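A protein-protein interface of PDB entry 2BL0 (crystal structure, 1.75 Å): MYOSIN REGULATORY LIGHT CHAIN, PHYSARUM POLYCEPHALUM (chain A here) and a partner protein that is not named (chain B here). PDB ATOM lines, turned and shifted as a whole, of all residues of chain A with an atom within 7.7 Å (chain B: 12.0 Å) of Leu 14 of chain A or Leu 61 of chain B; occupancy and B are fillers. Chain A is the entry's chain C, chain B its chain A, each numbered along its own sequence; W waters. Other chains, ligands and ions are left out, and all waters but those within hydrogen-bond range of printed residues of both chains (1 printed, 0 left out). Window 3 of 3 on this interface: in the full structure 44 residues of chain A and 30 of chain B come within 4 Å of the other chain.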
ATOM      1  N   PHE A   8      34.517 -19.726  -4.885  1.00  0.00           N
ATOM      2  CA  PHE A   8      33.252 -19.035  -5.128  1.00  0.00           C
ATOM      3  C   PHE A   8      33.274 -18.314  -6.458  1.00  0.00           C
ATOM      4  O   PHE A   8      32.270 -18.274  -7.138  1.00  0.00           O
ATOM      5  CB  PHE A   8      32.893 -18.070  -4.003  1.00  0.00           C
ATOM      6  CG  PHE A   8      32.554 -18.749  -2.714  1.00  0.00           C
ATOM      7  CD1 PHE A   8      31.817 -19.933  -2.699  1.00  0.00           C
ATOM      8  CD2 PHE A   8      32.990 -18.221  -1.509  1.00  0.00           C
ATOM      9  CE1 PHE A   8      31.517 -20.552  -1.507  1.00  0.00           C
ATOM     10  CE2 PHE A   8      32.684 -18.840  -0.336  1.00  0.00           C
ATOM     11  CZ  PHE A   8      31.944 -20.012  -0.341  1.00  0.00           C
ATOM     12  N   LYS A   9      34.424 -17.786  -6.848  1.00  0.00           N
ATOM     13  CA  LYS A   9      34.543 -17.092  -8.126  1.00  0.00           C
ATOM     14  C   LYS A   9      34.394 -18.093  -9.273  1.00  0.00           C
ATOM     15  O   LYS A   9      33.701 -17.814 -10.237  1.00  0.00           O
ATOM     16  CB  LYS A   9      35.876 -16.320  -8.212  1.00  0.00           C
ATOM     17  CG  LYS A   9      36.118 -15.549  -9.513  1.00  0.00           C
ATOM     18  CD  LYS A   9      35.182 -14.374  -9.674  1.00  0.00           C
ATOM     19  CE  LYS A   9      35.347 -13.670 -11.021  1.00  0.00           C
ATOM     20  NZ  LYS A   9      34.021 -13.355 -11.628  1.00  0.00           N
ATOM     21  N   GLU A  10      35.013 -19.267  -9.139  1.00  0.00           N
ATOM     22  CA  GLU A  10      34.898 -20.313 -10.149  1.00  0.00           C
ATOM     23  C   GLU A  10      33.437 -20.733 -10.328  1.00  0.00           C
ATOM     24  O   GLU A  10      32.970 -20.888 -11.446  1.00  0.00           O
ATOM     25  CB  GLU A  10      35.795 -21.514  -9.799  1.00  0.00           C
ATOM     26  CG  GLU A  10      37.273 -21.231 -10.002  1.00  0.00           C
ATOM     27  CD  GLU A  10      38.200 -22.271  -9.394  1.00  0.00           C
ATOM     28  OE1 GLU A  10      37.717 -23.208  -8.732  1.00  0.00           O
ATOM     29  OE2 GLU A  10      39.435 -22.142  -9.584  1.00  0.00           O
ATOM     30  N   ALA A  11      32.711 -20.877  -9.222  1.00  0.00           N
ATOM     31  CA  ALA A  11      31.299 -21.242  -9.262  1.00  0.00           C
ATOM     32  C   ALA A  11      30.489 -20.166  -9.945  1.00  0.00           C
ATOM     33  O   ALA A  11      29.644 -20.455 -10.783  1.00  0.00           O
ATOM     34  CB  ALA A  11      30.766 -21.487  -7.875  1.00  0.00           C
ATOM     35  N   PHE A  12      30.714 -18.910  -9.553  1.00  0.00           N
ATOM     36  CA  PHE A  12      30.004 -17.797 -10.162  1.00  0.00           C
ATOM     37  C   PHE A  12      30.223 -17.799 -11.689  1.00  0.00           C
ATOM     38  O   PHE A  12      29.297 -17.569 -12.479  1.00  0.00           O
ATOM     39  CB  PHE A  12      30.475 -16.475  -9.556  1.00  0.00           C
ATOM     40  CG  PHE A  12      29.738 -15.274 -10.082  1.00  0.00           C
ATOM     41  CD1 PHE A  12      28.548 -14.872  -9.503  1.00  0.00           C
ATOM     42  CD2 PHE A  12      30.235 -14.568 -11.165  1.00  0.00           C
ATOM     43  CE1 PHE A  12      27.863 -13.759 -10.002  1.00  0.00           C
ATOM     44  CE2 PHE A  12      29.561 -13.472 -11.680  1.00  0.00           C
ATOM     45  CZ  PHE A  12      28.372 -13.066 -11.084  1.00  0.00           C
ATOM     46  N   GLU A  13      31.464 -18.038 -12.092  1.00  0.00           N
ATOM     47  CA  GLU A  13      31.818 -18.071 -13.509  1.00  0.00           C
ATOM     48  C   GLU A  13      31.018 -19.165 -14.234  1.00  0.00           C
ATOM     49  O   GLU A  13      30.552 -18.954 -15.351  1.00  0.00           O
ATOM     50  CB  GLU A  13      33.325 -18.281 -13.699  1.00  0.00           C
ATOM     51  CG  GLU A  13      34.162 -17.043 -13.405  1.00  0.00           C
ATOM     52  CD  GLU A  13      33.735 -15.849 -14.226  1.00  0.00           C
ATOM     53  OE1 GLU A  13      33.953 -15.856 -15.451  1.00  0.00           O
ATOM     54  OE2 GLU A  13      33.155 -14.921 -13.640  1.00  0.00           O
ATOM     55  N   LEU A  14      30.845 -20.320 -13.603  1.00  0.00           N
ATOM     56  CA  LEU A  14      30.052 -21.399 -14.212  1.00  0.00           C
ATOM     57  C   LEU A  14      28.606 -20.977 -14.326  1.00  0.00           C
ATOM     58  O   LEU A  14      27.935 -21.298 -15.310  1.00  0.00           O
ATOM     59  CB  LEU A  14      30.111 -22.704 -13.395  1.00  0.00           C
ATOM     60  CG  LEU A  14      31.365 -23.557 -13.472  1.00  0.00           C
ATOM     61  CD1 LEU A  14      31.079 -24.917 -12.826  1.00  0.00           C
ATOM     62  CD2 LEU A  14      31.858 -23.735 -14.911  1.00  0.00           C
ATOM     63  N   PHE A  15      28.118 -20.229 -13.334  1.00  0.00           N
ATOM     64  CA  PHE A  15      26.744 -19.736 -13.347  1.00  0.00           C
ATOM     65  C   PHE A  15      26.546 -18.545 -14.310  1.00  0.00           C
ATOM     66  O   PHE A  15      25.405 -18.110 -14.525  1.00  0.00           O
ATOM     67  CB  PHE A  15      26.289 -19.328 -11.942  1.00  0.00           C
ATOM     68  CG  PHE A  15      26.431 -20.425 -10.895  1.00  0.00           C
ATOM     69  CD1 PHE A  15      26.414 -21.782 -11.244  1.00  0.00           C
ATOM     70  CD2 PHE A  15      26.588 -20.095  -9.562  1.00  0.00           C
ATOM     71  CE1 PHE A  15      26.570 -22.760 -10.297  1.00  0.00           C
ATOM     72  CE2 PHE A  15      26.727 -21.070  -8.608  1.00  0.00           C
ATOM     73  CZ  PHE A  15      26.715 -22.402  -8.961  1.00  0.00           C
ATOM     74  N   ASP A  16      27.648 -18.005 -14.827  1.00  0.00           N
ATOM     75  CA  ASP A  16      27.645 -16.861 -15.737  1.00  0.00           C
ATOM     76  C   ASP A  16      27.990 -17.408 -17.136  1.00  0.00           C
ATOM     77  O   ASP A  16      28.934 -16.951 -17.793  1.00  0.00           O
ATOM     78  CB  ASP A  16      28.670 -15.817 -15.257  1.00  0.00           C
ATOM     79  CG  ASP A  16      28.796 -14.608 -16.185  1.00  0.00           C
ATOM     80  OD1 ASP A  16      27.808 -14.226 -16.836  1.00  0.00           O
ATOM     81  OD2 ASP A  16      29.853 -13.960 -16.310  1.00  0.00           O
ATOM     82  N   SER A  17      27.227 -18.399 -17.586  1.00  0.00           N
ATOM     83  CA  SER A  17      27.555 -19.080 -18.843  1.00  0.00           C
ATOM     84  C   SER A  17      27.168 -18.258 -20.086  1.00  0.00           C
ATOM     85  O   SER A  17      27.483 -18.643 -21.211  1.00  0.00           O
ATOM     86  CB  SER A  17      26.987 -20.514 -18.891  1.00  0.00           C
ATOM     87  OG  SER A  17      25.582 -20.566 -18.745  1.00  0.00           O
ATOM     88  N   GLU A  18      26.492 -17.129 -19.879  1.00  0.00           N
ATOM     89  CA  GLU A  18      26.365 -16.109 -20.924  1.00  0.00           C
ATOM     90  C   GLU A  18      27.512 -15.072 -20.951  1.00  0.00           C
ATOM     91  O   GLU A  18      27.603 -14.289 -21.896  1.00  0.00           O
ATOM     92  CB  GLU A  18      25.027 -15.398 -20.802  1.00  0.00           C
ATOM     93  CG  GLU A  18      23.876 -16.178 -21.396  1.00  0.00           C
ATOM     94  CD  GLU A  18      22.689 -15.277 -21.692  1.00  0.00           C
ATOM     95  OE1 GLU A  18      21.703 -15.334 -20.935  1.00  0.00           O
ATOM     96  OE2 GLU A  18      22.752 -14.499 -22.670  1.00  0.00           O
ATOM     97  N   ILE A  23      24.263 -12.213 -12.926  1.00  0.00           N
ATOM     98  CA  ILE A  23      23.185 -13.188 -13.022  1.00  0.00           C
ATOM     99  C   ILE A  23      21.867 -12.501 -12.841  1.00  0.00           C
ATOM    100  O   ILE A  23      21.612 -11.920 -11.785  1.00  0.00           O
ATOM    101  CB  ILE A  23      23.320 -14.268 -11.950  1.00  0.00           C
ATOM    102  CG1 ILE A  23      24.693 -14.947 -12.040  1.00  0.00           C
ATOM    103  CG2 ILE A  23      22.136 -15.266 -12.057  1.00  0.00           C
ATOM    104  CD1 ILE A  23      25.000 -15.861 -10.881  1.00  0.00           C
ATOM    105  N   VAL A  31      20.166 -21.487 -14.914  1.00  0.00           N
ATOM    106  CA  VAL A  31      21.177 -22.163 -14.116  1.00  0.00           C
ATOM    107  C   VAL A  31      20.579 -23.299 -13.267  1.00  0.00           C
ATOM    108  O   VAL A  31      21.120 -24.421 -13.211  1.00  0.00           O
ATOM    109  CB  VAL A  31      21.921 -21.127 -13.206  1.00  0.00           C
ATOM    110  CG1 VAL A  31      22.767 -21.831 -12.198  1.00  0.00           C
ATOM    111  CG2 VAL A  31      22.777 -20.210 -14.079  1.00  0.00           C
ATOM    112  N   GLN A  34      19.827 -26.157 -15.502  1.00  0.00           N
ATOM    113  CA  GLN A  34      21.059 -26.810 -15.954  1.00  0.00           C
ATOM    114  C   GLN A  34      21.521 -27.818 -14.915  1.00  0.00           C
ATOM    115  O   GLN A  34      21.826 -28.977 -15.235  1.00  0.00           O
ATOM    116  CB  GLN A  34      22.184 -25.791 -16.202  1.00  0.00           C
ATOM    117  CG  GLN A  34      22.043 -24.877 -17.410  1.00  0.00           C
ATOM    118  CD  GLN A  34      23.160 -23.820 -17.480  1.00  0.00           C
ATOM    119  OE1 GLN A  34      23.767 -23.508 -16.467  1.00  0.00           O
ATOM    120  NE2 GLN A  34      23.410 -23.265 -18.679  1.00  0.00           N
ATOM    121  N   PHE A  35      21.558 -27.394 -13.651  1.00  0.00           N
ATOM    122  CA  PHE A  35      22.143 -28.220 -12.594  1.00  0.00           C
ATOM    123  C   PHE A  35      21.102 -29.120 -11.880  1.00  0.00           C
ATOM    124  O   PHE A  35      21.445 -29.884 -10.982  1.00  0.00           O
ATOM    125  CB  PHE A  35      22.874 -27.323 -11.583  1.00  0.00           C
ATOM    126  CG  PHE A  35      24.169 -26.754 -12.096  1.00  0.00           C
ATOM    127  CD1 PHE A  35      24.178 -25.556 -12.788  1.00  0.00           C
ATOM    128  CD2 PHE A  35      25.388 -27.434 -11.895  1.00  0.00           C
ATOM    129  CE1 PHE A  35      25.345 -25.033 -13.282  1.00  0.00           C
ATOM    130  CE2 PHE A  35      26.577 -26.888 -12.363  1.00  0.00           C
ATOM    131  CZ  PHE A  35      26.566 -25.696 -13.052  1.00  0.00           C
ATOM    132  N   TRP B  51      21.116 -22.163  -2.555  1.00  0.00           N
ATOM    133  CA  TRP B  51      22.422 -21.762  -3.086  1.00  0.00           C
ATOM    134  C   TRP B  51      23.489 -22.787  -2.769  1.00  0.00           C
ATOM    135  O   TRP B  51      24.411 -22.985  -3.553  1.00  0.00           O
ATOM    136  CB  TRP B  51      22.853 -20.388  -2.566  1.00  0.00           C
ATOM    137  CG  TRP B  51      22.215 -19.223  -3.266  1.00  0.00           C
ATOM    138  CD1 TRP B  51      21.282 -18.381  -2.745  1.00  0.00           C
ATOM    139  CD2 TRP B  51      22.438 -18.787  -4.617  1.00  0.00           C
ATOM    140  NE1 TRP B  51      20.920 -17.439  -3.671  1.00  0.00           N
ATOM    141  CE2 TRP B  51      21.618 -17.651  -4.830  1.00  0.00           C
ATOM    142  CE3 TRP B  51      23.278 -19.213  -5.661  1.00  0.00           C
ATOM    143  CZ2 TRP B  51      21.591 -16.948  -6.048  1.00  0.00           C
ATOM    144  CZ3 TRP B  51      23.259 -18.514  -6.866  1.00  0.00           C
ATOM    145  CH2 TRP B  51      22.403 -17.395  -7.058  1.00  0.00           C
ATOM    146  N   TRP B  52      23.382 -23.408  -1.597  1.00  0.00           N
ATOM    147  CA  TRP B  52      24.231 -24.546  -1.267  1.00  0.00           C
ATOM    148  C   TRP B  52      24.036 -25.710  -2.218  1.00  0.00           C
ATOM    149  O   TRP B  52      25.012 -26.292  -2.672  1.00  0.00           O
ATOM    150  CB  TRP B  52      23.971 -25.032   0.156  1.00  0.00           C
ATOM    151  CG  TRP B  52      24.439 -26.442   0.385  1.00  0.00           C
ATOM    152  CD1 TRP B  52      23.667 -27.540   0.617  1.00  0.00           C
ATOM    153  CD2 TRP B  52      25.783 -26.887   0.387  1.00  0.00           C
ATOM    154  NE1 TRP B  52      24.459 -28.655   0.766  1.00  0.00           N
ATOM    155  CE2 TRP B  52      25.769 -28.277   0.629  1.00  0.00           C
ATOM    156  CE3 TRP B  52      27.019 -26.248   0.218  1.00  0.00           C
ATOM    157  CZ2 TRP B  52      26.935 -29.033   0.703  1.00  0.00           C
ATOM    158  CZ3 TRP B  52      28.170 -26.994   0.294  1.00  0.00           C
ATOM    159  CH2 TRP B  52      28.124 -28.370   0.536  1.00  0.00           C
ATOM    160  N   LYS B  53      22.783 -26.064  -2.509  1.00  0.00           N
ATOM    161  CA  LYS B  53      22.518 -27.218  -3.352  1.00  0.00           C
ATOM    162  C   LYS B  53      23.120 -27.000  -4.723  1.00  0.00           C
ATOM    163  O   LYS B  53      23.708 -27.902  -5.294  1.00  0.00           O
ATOM    164  CB  LYS B  53      21.018 -27.486  -3.464  1.00  0.00           C
ATOM    165  CG  LYS B  53      20.403 -27.965  -2.154  1.00  0.00           C
ATOM    166  CD  LYS B  53      18.934 -28.262  -2.320  1.00  0.00           C
ATOM    167  CE  LYS B  53      18.196 -28.138  -1.011  1.00  0.00           C
ATOM    168  NZ  LYS B  53      16.859 -28.744  -1.147  1.00  0.00           N
ATOM    169  N   LEU B  54      22.977 -25.782  -5.233  1.00  0.00           N
ATOM    170  CA  LEU B  54      23.537 -25.423  -6.506  1.00  0.00           C
ATOM    171  C   LEU B  54      25.067 -25.444  -6.453  1.00  0.00           C
ATOM    172  O   LEU B  54      25.710 -26.027  -7.330  1.00  0.00           O
ATOM    173  CB  LEU B  54      22.994 -24.050  -6.923  1.00  0.00           C
ATOM    174  CG  LEU B  54      23.452 -23.512  -8.248  1.00  0.00           C
ATOM    175  CD1 LEU B  54      22.980 -24.409  -9.387  1.00  0.00           C
ATOM    176  CD2 LEU B  54      22.892 -22.089  -8.382  1.00  0.00           C
ATOM    177  N   PHE B  55      25.646 -24.844  -5.419  1.00  0.00           N
ATOM    178  CA  PHE B  55      27.101 -24.794  -5.284  1.00  0.00           C
ATOM    179  C   PHE B  55      27.696 -26.196  -5.178  1.00  0.00           C
ATOM    180  O   PHE B  55      28.725 -26.482  -5.778  1.00  0.00           O
ATOM    181  CB  PHE B  55      27.502 -23.955  -4.068  1.00  0.00           C
ATOM    182  CG  PHE B  55      28.974 -23.933  -3.809  1.00  0.00           C
ATOM    183  CD1 PHE B  55      29.813 -23.195  -4.627  1.00  0.00           C
ATOM    184  CD2 PHE B  55      29.518 -24.647  -2.760  1.00  0.00           C
ATOM    185  CE1 PHE B  55      31.179 -23.170  -4.409  1.00  0.00           C
ATOM    186  CE2 PHE B  55      30.888 -24.629  -2.541  1.00  0.00           C
ATOM    187  CZ  PHE B  55      31.712 -23.886  -3.374  1.00  0.00           C
ATOM    188  N   ALA B  56      27.012 -27.065  -4.448  1.00  0.00           N
ATOM    189  CA  ALA B  56      27.462 -28.436  -4.235  1.00  0.00           C
ATOM    190  C   ALA B  56      27.435 -29.210  -5.540  1.00  0.00           C
ATOM    191  O   ALA B  56      28.314 -30.039  -5.779  1.00  0.00           O
ATOM    192  CB  ALA B  56      26.613 -29.107  -3.190  1.00  0.00           C
ATOM    193  N   LYS B  57      26.440 -28.925  -6.386  1.00  0.00           N
ATOM    194  CA  LYS B  57      26.351 -29.553  -7.700  1.00  0.00           C
ATOM    195  C   LYS B  57      27.466 -29.069  -8.615  1.00  0.00           C
ATOM    196  O   LYS B  57      27.993 -29.850  -9.413  1.00  0.00           O
ATOM    197  CB  LYS B  57      24.991 -29.307  -8.361  1.00  0.00           C
ATOM    198  CG  LYS B  57      23.882 -30.244  -7.897  1.00  0.00           C
ATOM    199  CD  LYS B  57      23.708 -31.434  -8.848  1.00  0.00           C
ATOM    200  CE  LYS B  57      22.337 -32.119  -8.715  1.00  0.00           C
ATOM    201  NZ  LYS B  57      21.407 -31.458  -7.742  1.00  0.00           N
ATOM    202  N   ALA B  58      27.819 -27.790  -8.508  1.00  0.00           N
ATOM    203  CA  ALA B  58      28.869 -27.208  -9.348  1.00  0.00           C
ATOM    204  C   ALA B  58      30.281 -27.605  -8.895  1.00  0.00           C
ATOM    205  O   ALA B  58      31.202 -27.614  -9.697  1.00  0.00           O
ATOM    206  CB  ALA B  58      28.746 -25.698  -9.372  1.00  0.00           C
ATOM    207  N   ARG B  59      30.445 -27.932  -7.613  1.00  0.00           N
ATOM    208  CA  ARG B  59      31.778 -28.071  -7.021  1.00  0.00           C
ATOM    209  C   ARG B  59      32.706 -29.052  -7.773  1.00  0.00           C
ATOM    210  O   ARG B  59      33.866 -28.735  -7.988  1.00  0.00           O
ATOM    211  CB  ARG B  59      31.687 -28.486  -5.542  1.00  0.00           C
ATOM    212  CG  ARG B  59      32.608 -27.671  -4.604  1.00  0.00           C
ATOM    213  CD  ARG B  59      32.882 -28.328  -3.231  1.00  0.00           C
ATOM    214  NE  ARG B  59      32.520 -27.498  -2.073  1.00  0.00           N
ATOM    215  CZ  ARG B  59      33.371 -26.856  -1.265  1.00  0.00           C
ATOM    216  NH1 ARG B  59      34.685 -26.891  -1.473  1.00  0.00           N
ATOM    217  NH2 ARG B  59      32.916 -26.141  -0.242  1.00  0.00           N
ATOM    218  N   PRO B  60      32.213 -30.224  -8.159  1.00  0.00           N
ATOM    219  CA  PRO B  60      33.028 -31.191  -8.919  1.00  0.00           C
ATOM    220  C   PRO B  60      33.528 -30.681 -10.264  1.00  0.00           C
ATOM    221  O   PRO B  60      34.466 -31.264 -10.817  1.00  0.00           O
ATOM    222  CB  PRO B  60      32.057 -32.360  -9.135  1.00  0.00           C
ATOM    223  CG  PRO B  60      31.148 -32.258  -7.968  1.00  0.00           C
ATOM    224  CD  PRO B  60      30.878 -30.770  -7.874  1.00  0.00           C
ATOM    225  N   LEU B  61      32.908 -29.630 -10.790  1.00  0.00           N
ATOM    226  CA  LEU B  61      33.319 -29.032 -12.065  1.00  0.00           C
ATOM    227  C   LEU B  61      34.427 -27.982 -11.898  1.00  0.00           C
ATOM    228  O   LEU B  61      34.978 -27.503 -12.886  1.00  0.00           O
ATOM    229  CB  LEU B  61      32.109 -28.398 -12.768  1.00  0.00           C
ATOM    230  CG  LEU B  61      31.228 -29.302 -13.634  1.00  0.00           C
ATOM    231  CD1 LEU B  61      30.822 -30.571 -12.943  1.00  0.00           C
ATOM    232  CD2 LEU B  61      30.012 -28.540 -14.120  1.00  0.00           C
ATOM    233  N   LEU B  62      34.759 -27.640 -10.654  1.00  0.00           N
ATOM    234  CA  LEU B  62      35.687 -26.555 -10.368  1.00  0.00           C
ATOM    235  C   LEU B  62      37.120 -27.072 -10.235  1.00  0.00           C
ATOM    236  O   LEU B  62      37.349 -28.182  -9.765  1.00  0.00           O
ATOM    237  CB  LEU B  62      35.262 -25.838  -9.078  1.00  0.00           C
ATOM    238  CG  LEU B  62      33.788 -25.429  -9.006  1.00  0.00           C
ATOM    239  CD1 LEU B  62      33.443 -24.699  -7.693  1.00  0.00           C
ATOM    240  CD2 LEU B  62      33.401 -24.590 -10.184  1.00  0.00           C
ATOM    241  N   VAL B  63      38.068 -26.238 -10.640  1.00  0.00           N
ATOM    242  CA  VAL B  63      39.482 -26.574 -10.599  1.00  0.00           C
ATOM    243  C   VAL B  63      39.967 -26.530  -9.157  1.00  0.00           C
ATOM    244  O   VAL B  63      40.581 -27.502  -8.681  1.00  0.00           O
ATOM    245  CB  VAL B  63      40.329 -25.620 -11.499  1.00  0.00           C
ATOM    246  CG1 VAL B  63      41.798 -26.040 -11.494  1.00  0.00           C
ATOM    247  CG2 VAL B  63      39.813 -25.573 -12.948  1.00  0.00           C
HETATM  248  O   HOH W   1      37.298 -23.780 -11.783  1.00  0.00           O
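Phe 55 of chain B touches Phe 8 of chain A (CE1 to CD1, 3.7 Å). OE1 of Glu 10 of chain A touches N of Val 63 of chain B, 3.6 Å away. CD1 of Phe 55 of chain B touches CB of Ala 11 of chain A, 3.8 Å away. Leu 14 of chain A touches Leu 62 of chain B (CD1 to CD2, 3.5 Å). Leu 54 of chain B touches Phe 15 of chain A (CG to CZ, 3.5 Å). Ala 58 of chain B touches Phe 15 of chain A. Leu 54 of chain B touches Val 31 of chain A (CD1 to CG1, 3.8 Å). CD1 of Leu 54 of chain B touches CB of Phe 35 of chain A, at 3.7 Å. Phe 35 of chain A touches Lys 57 of chain B (O to CE, 3.3 Å). Phe 35 of chain A touches Ala 58 of chain B (CE2 to CA, 3.8 Å).
Of chain B, only Leu 61 and Leu 62 come within 4 Å of Leu 14 of chain A. Leu 61 of chain B touches one residue of chain A. Glu 10 of chain A touches just these residues of chain B: Leu 62 and Val 63. Printed residues of chain B within 4 Å of Ala 11 of chain A: Phe 55 and Leu 62. No residue of chain B comes within 4 Å of Glu 13 of chain A. No residue of chain B comes within 4 Å of Ser 17 of chain A. Printed residues of chain A within 4 Å of Val 63 of chain B: Glu 10. Printed residues of chain B within 4 Å of Phe 8 of chain A: Phe 55 (3.7 Å). Ala 56 of chain B touches none of the printed residues of chain A. Arg 59 of chain B touches none of the printed residues of chain A. The nearest residue of chain B that does not touch Leu 14 of chain A is Ala 58 of chain B (4.1 Å). The nearest residue of chain A that does not touch Leu 61 of chain B is Phe 35 of chain A (4.2 Å).
Water W1 lies within hydrogen-bond range of N of Val 63 of chain B (2.8 Å) and OE1 of Glu 10 of chain A (3.1 Å).
Of the 13 printed residues of chain B, 7 touch a printed residue of chain A. Printed residues of chain A that touch a printed residue of chain B: Phe 8, Glu 10, Ala 11, Leu 14, Phe 15, Val 31 and Phe 35. Hydrophobic or aromatic side chains of chain A within 4 Å of the printed part of chain B: Phe 8, Ala 11, Leu 14, Phe 15, Val 31 and Phe 35. Among the printed residues, no Asp or Glu carboxylate lies within 4 Å of a Lys or Arg side-chain nitrogen of the other chain.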
